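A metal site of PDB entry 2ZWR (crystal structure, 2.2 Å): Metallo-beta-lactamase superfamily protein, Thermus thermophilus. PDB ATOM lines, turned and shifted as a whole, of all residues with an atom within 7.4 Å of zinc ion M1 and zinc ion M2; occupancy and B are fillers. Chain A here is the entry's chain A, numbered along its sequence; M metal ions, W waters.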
ATOM      1  N   LEU A  11      -7.907   2.515   7.516  1.00  0.00           N
ATOM      2  CA  LEU A  11      -9.164   1.807   7.371  1.00  0.00           C
ATOM      3  C   LEU A  11      -9.125   0.857   6.173  1.00  0.00           C
ATOM      4  O   LEU A  11     -10.123   0.249   5.808  1.00  0.00           O
ATOM      5  CB  LEU A  11     -10.364   2.770   7.291  1.00  0.00           C
ATOM      6  CG  LEU A  11     -10.983   3.345   8.591  1.00  0.00           C
ATOM      7  CD1 LEU A  11     -11.277   2.242   9.623  1.00  0.00           C
ATOM      8  CD2 LEU A  11     -10.125   4.426   9.240  1.00  0.00           C
ATOM      9  N   GLN A  12      -7.938   0.725   5.567  1.00  0.00           N
ATOM     10  CA  GLN A  12      -7.686  -0.244   4.509  1.00  0.00           C
ATOM     11  C   GLN A  12      -8.755  -0.192   3.406  1.00  0.00           C
ATOM     12  O   GLN A  12      -9.475  -1.172   3.141  1.00  0.00           O
ATOM     13  CB  GLN A  12      -7.527  -1.635   5.117  1.00  0.00           C
ATOM     14  CG  GLN A  12      -6.230  -1.784   5.916  1.00  0.00           C
ATOM     15  CD  GLN A  12      -6.071  -3.132   6.576  1.00  0.00           C
ATOM     16  OE1 GLN A  12      -7.044  -3.746   7.028  1.00  0.00           O
ATOM     17  NE2 GLN A  12      -4.828  -3.597   6.646  1.00  0.00           N
ATOM     18  N   GLU A  13      -8.866   0.975   2.789  1.00  0.00           N
ATOM     19  CA  GLU A  13      -9.868   1.250   1.779  1.00  0.00           C
ATOM     20  C   GLU A  13      -9.261   0.988   0.408  1.00  0.00           C
ATOM     21  O   GLU A  13      -8.062   1.221   0.218  1.00  0.00           O
ATOM     22  CB  GLU A  13     -10.347   2.699   1.926  1.00  0.00           C
ATOM     23  CG  GLU A  13     -11.311   3.207   0.838  1.00  0.00           C
ATOM     24  CD  GLU A  13     -10.600   3.938  -0.295  1.00  0.00           C
ATOM     25  OE1 GLU A  13      -9.380   4.161  -0.224  1.00  0.00           O
ATOM     26  OE2 GLU A  13     -11.279   4.281  -1.286  1.00  0.00           O
ATOM     27  N   ASN A  14     -10.065   0.494  -0.537  1.00  0.00           N
ATOM     28  CA  ASN A  14      -9.591   0.240  -1.903  1.00  0.00           C
ATOM     29  C   ASN A  14      -9.908   1.368  -2.913  1.00  0.00           C
ATOM     30  O   ASN A  14     -11.092   1.657  -3.195  1.00  0.00           O
ATOM     31  CB  ASN A  14     -10.165  -1.082  -2.468  1.00  0.00           C
ATOM     32  CG  ASN A  14      -9.931  -2.292  -1.552  1.00  0.00           C
ATOM     33  OD1 ASN A  14     -10.793  -3.173  -1.462  1.00  0.00           O
ATOM     34  ND2 ASN A  14      -8.774  -2.355  -0.900  1.00  0.00           N
ATOM     35  N   ASP A  28     -12.368   6.628  -5.681  1.00  0.00           N
ATOM     36  CA  ASP A  28     -12.188   6.664  -4.208  1.00  0.00           C
ATOM     37  C   ASP A  28     -10.725   6.771  -3.715  1.00  0.00           C
ATOM     38  O   ASP A  28     -10.240   5.870  -3.004  1.00  0.00           O
ATOM     39  CB  ASP A  28     -12.865   5.451  -3.532  1.00  0.00           C
ATOM     40  CG  ASP A  28     -14.371   5.410  -3.715  1.00  0.00           C
ATOM     41  OD1 ASP A  28     -14.958   6.334  -4.329  1.00  0.00           O
ATOM     42  OD2 ASP A  28     -14.979   4.427  -3.237  1.00  0.00           O
ATOM     43  N   THR A  53     -17.699   6.755  -5.054  1.00  0.00           N
ATOM     44  CA  THR A  53     -18.836   5.903  -4.712  1.00  0.00           C
ATOM     45  C   THR A  53     -19.601   6.539  -3.574  1.00  0.00           C
ATOM     46  O   THR A  53     -20.832   6.536  -3.581  1.00  0.00           O
ATOM     47  CB  THR A  53     -18.433   4.453  -4.291  1.00  0.00           C
ATOM     48  OG1 THR A  53     -17.669   4.501  -3.067  1.00  0.00           O
ATOM     49  CG2 THR A  53     -17.660   3.729  -5.409  1.00  0.00           C
ATOM     50  N   HIS A  54     -18.867   7.110  -2.622  1.00  0.00           N
ATOM     51  CA  HIS A  54     -19.474   7.896  -1.530  1.00  0.00           C
ATOM     52  C   HIS A  54     -18.399   8.734  -0.826  1.00  0.00           C
ATOM     53  O   HIS A  54     -17.230   8.674  -1.203  1.00  0.00           O
ATOM     54  CB  HIS A  54     -20.261   6.994  -0.574  1.00  0.00           C
ATOM     55  CG  HIS A  54     -19.403   6.038   0.230  1.00  0.00           C
ATOM     56  ND1 HIS A  54     -18.632   5.057  -0.348  1.00  0.00           N
ATOM     57  CD2 HIS A  54     -19.241   5.896   1.565  1.00  0.00           C
ATOM     58  CE1 HIS A  54     -18.018   4.364   0.589  1.00  0.00           C
ATOM     59  NE2 HIS A  54     -18.374   4.854   1.761  1.00  0.00           N
ATOM     60  N   ALA A  55     -18.805   9.501   0.188  1.00  0.00           N
ATOM     61  CA  ALA A  55     -17.926  10.507   0.814  1.00  0.00           C
ATOM     62  C   ALA A  55     -17.625  10.289   2.293  1.00  0.00           C
ATOM     63  O   ALA A  55     -17.323  11.254   3.000  1.00  0.00           O
ATOM     64  CB  ALA A  55     -18.460  11.906   0.586  1.00  0.00           C
ATOM     65  N   HIS A  56     -17.677   9.053   2.773  1.00  0.00           N
ATOM     66  CA  HIS A  56     -17.016   8.761   4.039  1.00  0.00           C
ATOM     67  C   HIS A  56     -15.523   9.111   3.916  1.00  0.00           C
ATOM     68  O   HIS A  56     -14.913   8.959   2.842  1.00  0.00           O
ATOM     69  CB  HIS A  56     -17.178   7.303   4.453  1.00  0.00           C
ATOM     70  CG  HIS A  56     -18.549   6.978   4.902  1.00  0.00           C
ATOM     71  ND1 HIS A  56     -19.084   5.710   4.781  1.00  0.00           N
ATOM     72  CD2 HIS A  56     -19.516   7.750   5.464  1.00  0.00           C
ATOM     73  CE1 HIS A  56     -20.325   5.713   5.255  1.00  0.00           C
ATOM     74  NE2 HIS A  56     -20.607   6.936   5.679  1.00  0.00           N
ATOM     75  N   PHE A  57     -14.964   9.607   5.021  1.00  0.00           N
ATOM     76  CA  PHE A  57     -13.592  10.121   5.035  1.00  0.00           C
ATOM     77  C   PHE A  57     -12.526   9.146   4.538  1.00  0.00           C
ATOM     78  O   PHE A  57     -11.505   9.590   3.995  1.00  0.00           O
ATOM     79  CB  PHE A  57     -13.227  10.691   6.421  1.00  0.00           C
ATOM     80  CG  PHE A  57     -12.998   9.654   7.505  1.00  0.00           C
ATOM     81  CD1 PHE A  57     -13.976   9.412   8.462  1.00  0.00           C
ATOM     82  CD2 PHE A  57     -11.782   8.966   7.610  1.00  0.00           C
ATOM     83  CE1 PHE A  57     -13.774   8.472   9.491  1.00  0.00           C
ATOM     84  CE2 PHE A  57     -11.559   8.027   8.631  1.00  0.00           C
ATOM     85  CZ  PHE A  57     -12.566   7.780   9.575  1.00  0.00           C
ATOM     86  N   ASP A  58     -12.747   7.845   4.716  1.00  0.00           N
ATOM     87  CA  ASP A  58     -11.781   6.846   4.244  1.00  0.00           C
ATOM     88  C   ASP A  58     -11.759   6.684   2.718  1.00  0.00           C
ATOM     89  O   ASP A  58     -10.914   5.985   2.168  1.00  0.00           O
ATOM     90  CB  ASP A  58     -11.967   5.484   4.953  1.00  0.00           C
ATOM     91  CG  ASP A  58     -13.370   4.911   4.784  1.00  0.00           C
ATOM     92  OD1 ASP A  58     -14.365   5.643   5.002  1.00  0.00           O
ATOM     93  OD2 ASP A  58     -13.492   3.725   4.433  1.00  0.00           O
ATOM     94  N   HIS A  59     -12.685   7.362   2.039  1.00  0.00           N
ATOM     95  CA  HIS A  59     -12.764   7.310   0.581  1.00  0.00           C
ATOM     96  C   HIS A  59     -12.310   8.613  -0.097  1.00  0.00           C
ATOM     97  O   HIS A  59     -12.166   8.658  -1.316  1.00  0.00           O
ATOM     98  CB  HIS A  59     -14.172   6.888   0.131  1.00  0.00           C
ATOM     99  CG  HIS A  59     -14.506   5.474   0.496  1.00  0.00           C
ATOM    100  ND1 HIS A  59     -14.501   4.442  -0.411  1.00  0.00           N
ATOM    101  CD2 HIS A  59     -14.789   4.916   1.699  1.00  0.00           C
ATOM    102  CE1 HIS A  59     -14.787   3.305   0.198  1.00  0.00           C
ATOM    103  NE2 HIS A  59     -14.952   3.561   1.483  1.00  0.00           N
ATOM    104  N   HIS A 125     -25.721   2.661   2.925  1.00  0.00           N
ATOM    105  CA  HIS A 125     -24.458   2.835   3.660  1.00  0.00           C
ATOM    106  C   HIS A 125     -24.209   4.344   3.842  1.00  0.00           C
ATOM    107  O   HIS A 125     -23.711   4.789   4.889  1.00  0.00           O
ATOM    108  CB  HIS A 125     -23.314   2.134   2.927  1.00  0.00           C
ATOM    109  CG  HIS A 125     -21.971   2.294   3.571  1.00  0.00           C
ATOM    110  ND1 HIS A 125     -21.566   1.563   4.658  1.00  0.00           N
ATOM    111  CD2 HIS A 125     -20.919   3.091   3.252  1.00  0.00           C
ATOM    112  CE1 HIS A 125     -20.341   1.901   5.004  1.00  0.00           C
ATOM    113  NE2 HIS A 125     -19.920   2.832   4.156  1.00  0.00           N
ATOM    114  N   SER A 126     -24.585   5.126   2.828  1.00  0.00           N
ATOM    115  CA  SER A 126     -24.635   6.582   2.907  1.00  0.00           C
ATOM    116  C   SER A 126     -25.694   7.070   1.906  1.00  0.00           C
ATOM    117  O   SER A 126     -26.039   6.350   0.986  1.00  0.00           O
ATOM    118  CB  SER A 126     -23.253   7.213   2.619  1.00  0.00           C
ATOM    119  OG  SER A 126     -22.916   7.090   1.252  1.00  0.00           O
ATOM    120  N   HIS A 129     -24.627   7.192  -1.866  1.00  0.00           N
ATOM    121  CA  HIS A 129     -23.764   6.070  -2.239  1.00  0.00           C
ATOM    122  C   HIS A 129     -24.168   5.568  -3.624  1.00  0.00           C
ATOM    123  O   HIS A 129     -25.342   5.232  -3.851  1.00  0.00           O
ATOM    124  CB  HIS A 129     -23.853   4.936  -1.209  1.00  0.00           C
ATOM    125  CG  HIS A 129     -22.743   3.932  -1.314  1.00  0.00           C
ATOM    126  ND1 HIS A 129     -22.577   3.120  -2.416  1.00  0.00           N
ATOM    127  CD2 HIS A 129     -21.734   3.622  -0.460  1.00  0.00           C
ATOM    128  CE1 HIS A 129     -21.509   2.352  -2.237  1.00  0.00           C
ATOM    129  NE2 HIS A 129     -20.991   2.633  -1.060  1.00  0.00           N
ATOM    130  N   GLY A 143     -18.357   0.278  -4.145  1.00  0.00           N
ATOM    131  CA  GLY A 143     -17.997   0.884  -2.870  1.00  0.00           C
ATOM    132  C   GLY A 143     -18.237  -0.022  -1.679  1.00  0.00           C
ATOM    133  O   GLY A 143     -17.815  -1.183  -1.669  1.00  0.00           O
ATOM    134  N   ASP A 144     -18.918   0.510  -0.674  1.00  0.00           N
ATOM    135  CA  ASP A 144     -19.129  -0.240   0.558  1.00  0.00           C
ATOM    136  C   ASP A 144     -20.513  -0.880   0.631  1.00  0.00           C
ATOM    137  O   ASP A 144     -21.042  -1.076   1.719  1.00  0.00           O
ATOM    138  CB  ASP A 144     -18.890   0.651   1.778  1.00  0.00           C
ATOM    139  CG  ASP A 144     -17.451   1.132   1.889  1.00  0.00           C
ATOM    140  OD1 ASP A 144     -16.618   0.750   1.022  1.00  0.00           O
ATOM    141  OD2 ASP A 144     -17.156   1.906   2.842  1.00  0.00           O
ATOM    142  N   LEU A 145     -21.108  -1.205  -0.524  1.00  0.00           N
ATOM    143  CA  LEU A 145     -22.393  -1.938  -0.543  1.00  0.00           C
ATOM    144  C   LEU A 145     -22.177  -3.413  -0.147  1.00  0.00           C
ATOM    145  O   LEU A 145     -22.751  -3.908   0.826  1.00  0.00           O
ATOM    146  CB  LEU A 145     -23.036  -1.877  -1.932  1.00  0.00           C
ATOM    147  CG  LEU A 145     -24.046  -0.758  -2.222  1.00  0.00           C
ATOM    148  N   PHE A 147     -19.352  -6.687   0.282  1.00  0.00           N
ATOM    149  CA  PHE A 147     -18.002  -7.198   0.466  1.00  0.00           C
ATOM    150  C   PHE A 147     -17.951  -8.699   0.191  1.00  0.00           C
ATOM    151  O   PHE A 147     -18.980  -9.333  -0.007  1.00  0.00           O
ATOM    152  CB  PHE A 147     -17.474  -6.903   1.878  1.00  0.00           C
ATOM    153  CG  PHE A 147     -17.498  -5.433   2.234  1.00  0.00           C
ATOM    154  CD1 PHE A 147     -17.035  -4.470   1.323  1.00  0.00           C
ATOM    155  CD2 PHE A 147     -17.982  -5.006   3.458  1.00  0.00           C
ATOM    156  CE1 PHE A 147     -17.054  -3.101   1.640  1.00  0.00           C
ATOM    157  CE2 PHE A 147     -18.009  -3.655   3.788  1.00  0.00           C
ATOM    158  CZ  PHE A 147     -17.525  -2.692   2.869  1.00  0.00           C
ATOM    159  N   GLY A 152     -21.794  -3.530   3.675  1.00  0.00           N
ATOM    160  CA  GLY A 152     -21.411  -2.264   4.305  1.00  0.00           C
ATOM    161  C   GLY A 152     -22.050  -2.060   5.664  1.00  0.00           C
ATOM    162  O   GLY A 152     -23.192  -2.465   5.887  1.00  0.00           O
ATOM    163  N   ARG A 153     -21.298  -1.454   6.579  1.00  0.00           N
ATOM    164  CA  ARG A 153     -21.840  -0.999   7.863  1.00  0.00           C
ATOM    165  C   ARG A 153     -23.077  -0.136   7.635  1.00  0.00           C
ATOM    166  O   ARG A 153     -23.127   0.662   6.684  1.00  0.00           O
ATOM    167  CB  ARG A 153     -20.797  -0.206   8.656  1.00  0.00           C
ATOM    168  CG  ARG A 153     -19.613  -1.047   9.140  1.00  0.00           C
ATOM    169  CD  ARG A 153     -18.582  -0.206   9.880  1.00  0.00           C
ATOM    170  NE  ARG A 153     -19.052   0.213  11.200  1.00  0.00           N
ATOM    171  CZ  ARG A 153     -18.349   0.919  12.078  1.00  0.00           C
ATOM    172  NH1 ARG A 153     -17.121   1.319  11.793  1.00  0.00           N
ATOM    173  NH2 ARG A 153     -18.877   1.238  13.259  1.00  0.00           N
ATOM    174  N   LEU A 156     -23.028   3.894  10.405  1.00  0.00           N
ATOM    175  CA  LEU A 156     -22.192   5.081  10.174  1.00  0.00           C
ATOM    176  C   LEU A 156     -23.040   6.309   9.836  1.00  0.00           C
ATOM    177  O   LEU A 156     -24.256   6.199   9.669  1.00  0.00           O
ATOM    178  CB  LEU A 156     -21.170   4.808   9.067  1.00  0.00           C
ATOM    179  CG  LEU A 156     -19.978   3.905   9.411  1.00  0.00           C
ATOM    180  CD1 LEU A 156     -19.089   3.716   8.189  1.00  0.00           C
ATOM    181  CD2 LEU A 156     -19.192   4.480  10.584  1.00  0.00           C
ATOM    182  N   PRO A 157     -22.403   7.509   9.797  1.00  0.00           N
ATOM    183  CA  PRO A 157     -23.115   8.738   9.402  1.00  0.00           C
ATOM    184  C   PRO A 157     -23.821   8.626   8.054  1.00  0.00           C
ATOM    185  O   PRO A 157     -23.199   8.259   7.028  1.00  0.00           O
ATOM    186  CB  PRO A 157     -21.996   9.792   9.364  1.00  0.00           C
ATOM    187  CG  PRO A 157     -21.008   9.308  10.367  1.00  0.00           C
ATOM    188  CD  PRO A 157     -21.003   7.800  10.172  1.00  0.00           C
ATOM    189  N   GLY A 183     -15.125  -1.335  -1.729  1.00  0.00           N
ATOM    190  CA  GLY A 183     -14.355  -0.328  -1.002  1.00  0.00           C
ATOM    191  C   GLY A 183     -13.396  -0.855   0.049  1.00  0.00           C
ATOM    192  O   GLY A 183     -12.495  -0.143   0.464  1.00  0.00           O
ATOM    193  N   HIS A 184     -13.607  -2.093   0.502  1.00  0.00           N
ATOM    194  CA  HIS A 184     -12.738  -2.757   1.491  1.00  0.00           C
ATOM    195  C   HIS A 184     -12.657  -4.255   1.219  1.00  0.00           C
ATOM    196  O   HIS A 184     -13.609  -4.858   0.765  1.00  0.00           O
ATOM    197  CB  HIS A 184     -13.234  -2.540   2.934  1.00  0.00           C
ATOM    198  CG  HIS A 184     -13.486  -1.096   3.272  1.00  0.00           C
ATOM    199  ND1 HIS A 184     -12.528  -0.305   3.871  1.00  0.00           N
ATOM    200  CD2 HIS A 184     -14.554  -0.306   3.057  1.00  0.00           C
ATOM    201  CE1 HIS A 184     -13.011   0.926   4.014  1.00  0.00           C
ATOM    202  NE2 HIS A 184     -14.237   0.948   3.528  1.00  0.00           N
HETATM  203 ZN    ZN M   1     -15.236   2.643   3.361  1.00  0.00          ZN
HETATM  204 ZN    ZN M   2     -18.212   4.011   3.773  1.00  0.00          ZN
HETATM  205  O   HOH W   1     -16.292   3.774   4.493  1.00  0.00           O
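The backbone carbonyl oxygen (O) of Arg 153 lies within hydrogen-bond range of a ring nitrogen (ND1) of His 125.
A ring nitrogen (ND1) of His 54 sits close to a ring nitrogen (NE2) of His 129.
The backbone NH (N) of Asp 144 lies within hydrogen-bond range of a ring nitrogen (NE2) of His 129 (3.0 Å).
OE2 of Glu 13 is in hydrogen-bond range of ND1 of His 59 (3.3 Å).
The side-chain hydroxyl of Thr 53 is in hydrogen-bond range of a ring nitrogen (ND1) of His 54 (2.9 Å).
A ring nitrogen (ND1) of His 184 sits at hydrogen-bond distance from the backbone carbonyl oxygen (O) of Leu 11.
The backbone carbonyl oxygen (O) of Pro 157 sits at hydrogen-bond distance from a ring nitrogen (NE2) of His 56 (3.2 Å).
O of Gln 12 sits at hydrogen-bond distance from ND1 of His 184 (3.3 Å).
Within 4 Å of zinc ion M1: Asp 58, His 59, Asp 144 and His 184.
Zinc ion M1 is bound by water W1 (1.9 Å), a ring nitrogen (NE2) of His 184 (2.0 Å), a ring nitrogen (NE2) of His 59 (2.1 Å), the side-chain carboxylate of Asp 144 (2.1 Å) and the side-chain carboxylate of Asp 58 (2.3 Å).
Water W1 binds zinc ion M2 (2.1 Å).
Zinc ion M2 is bound by NE2 of His 125.
ND1 of His 56 is bound to zinc ion M2 (2.2 Å).
NE2 of His 54 is bound to zinc ion M2 (2.2 Å).
Zinc ion M2 is bound by OD2 of Asp 144, at 2.5 Å.
Zinc ion M2 has five donor atoms within binding distance.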
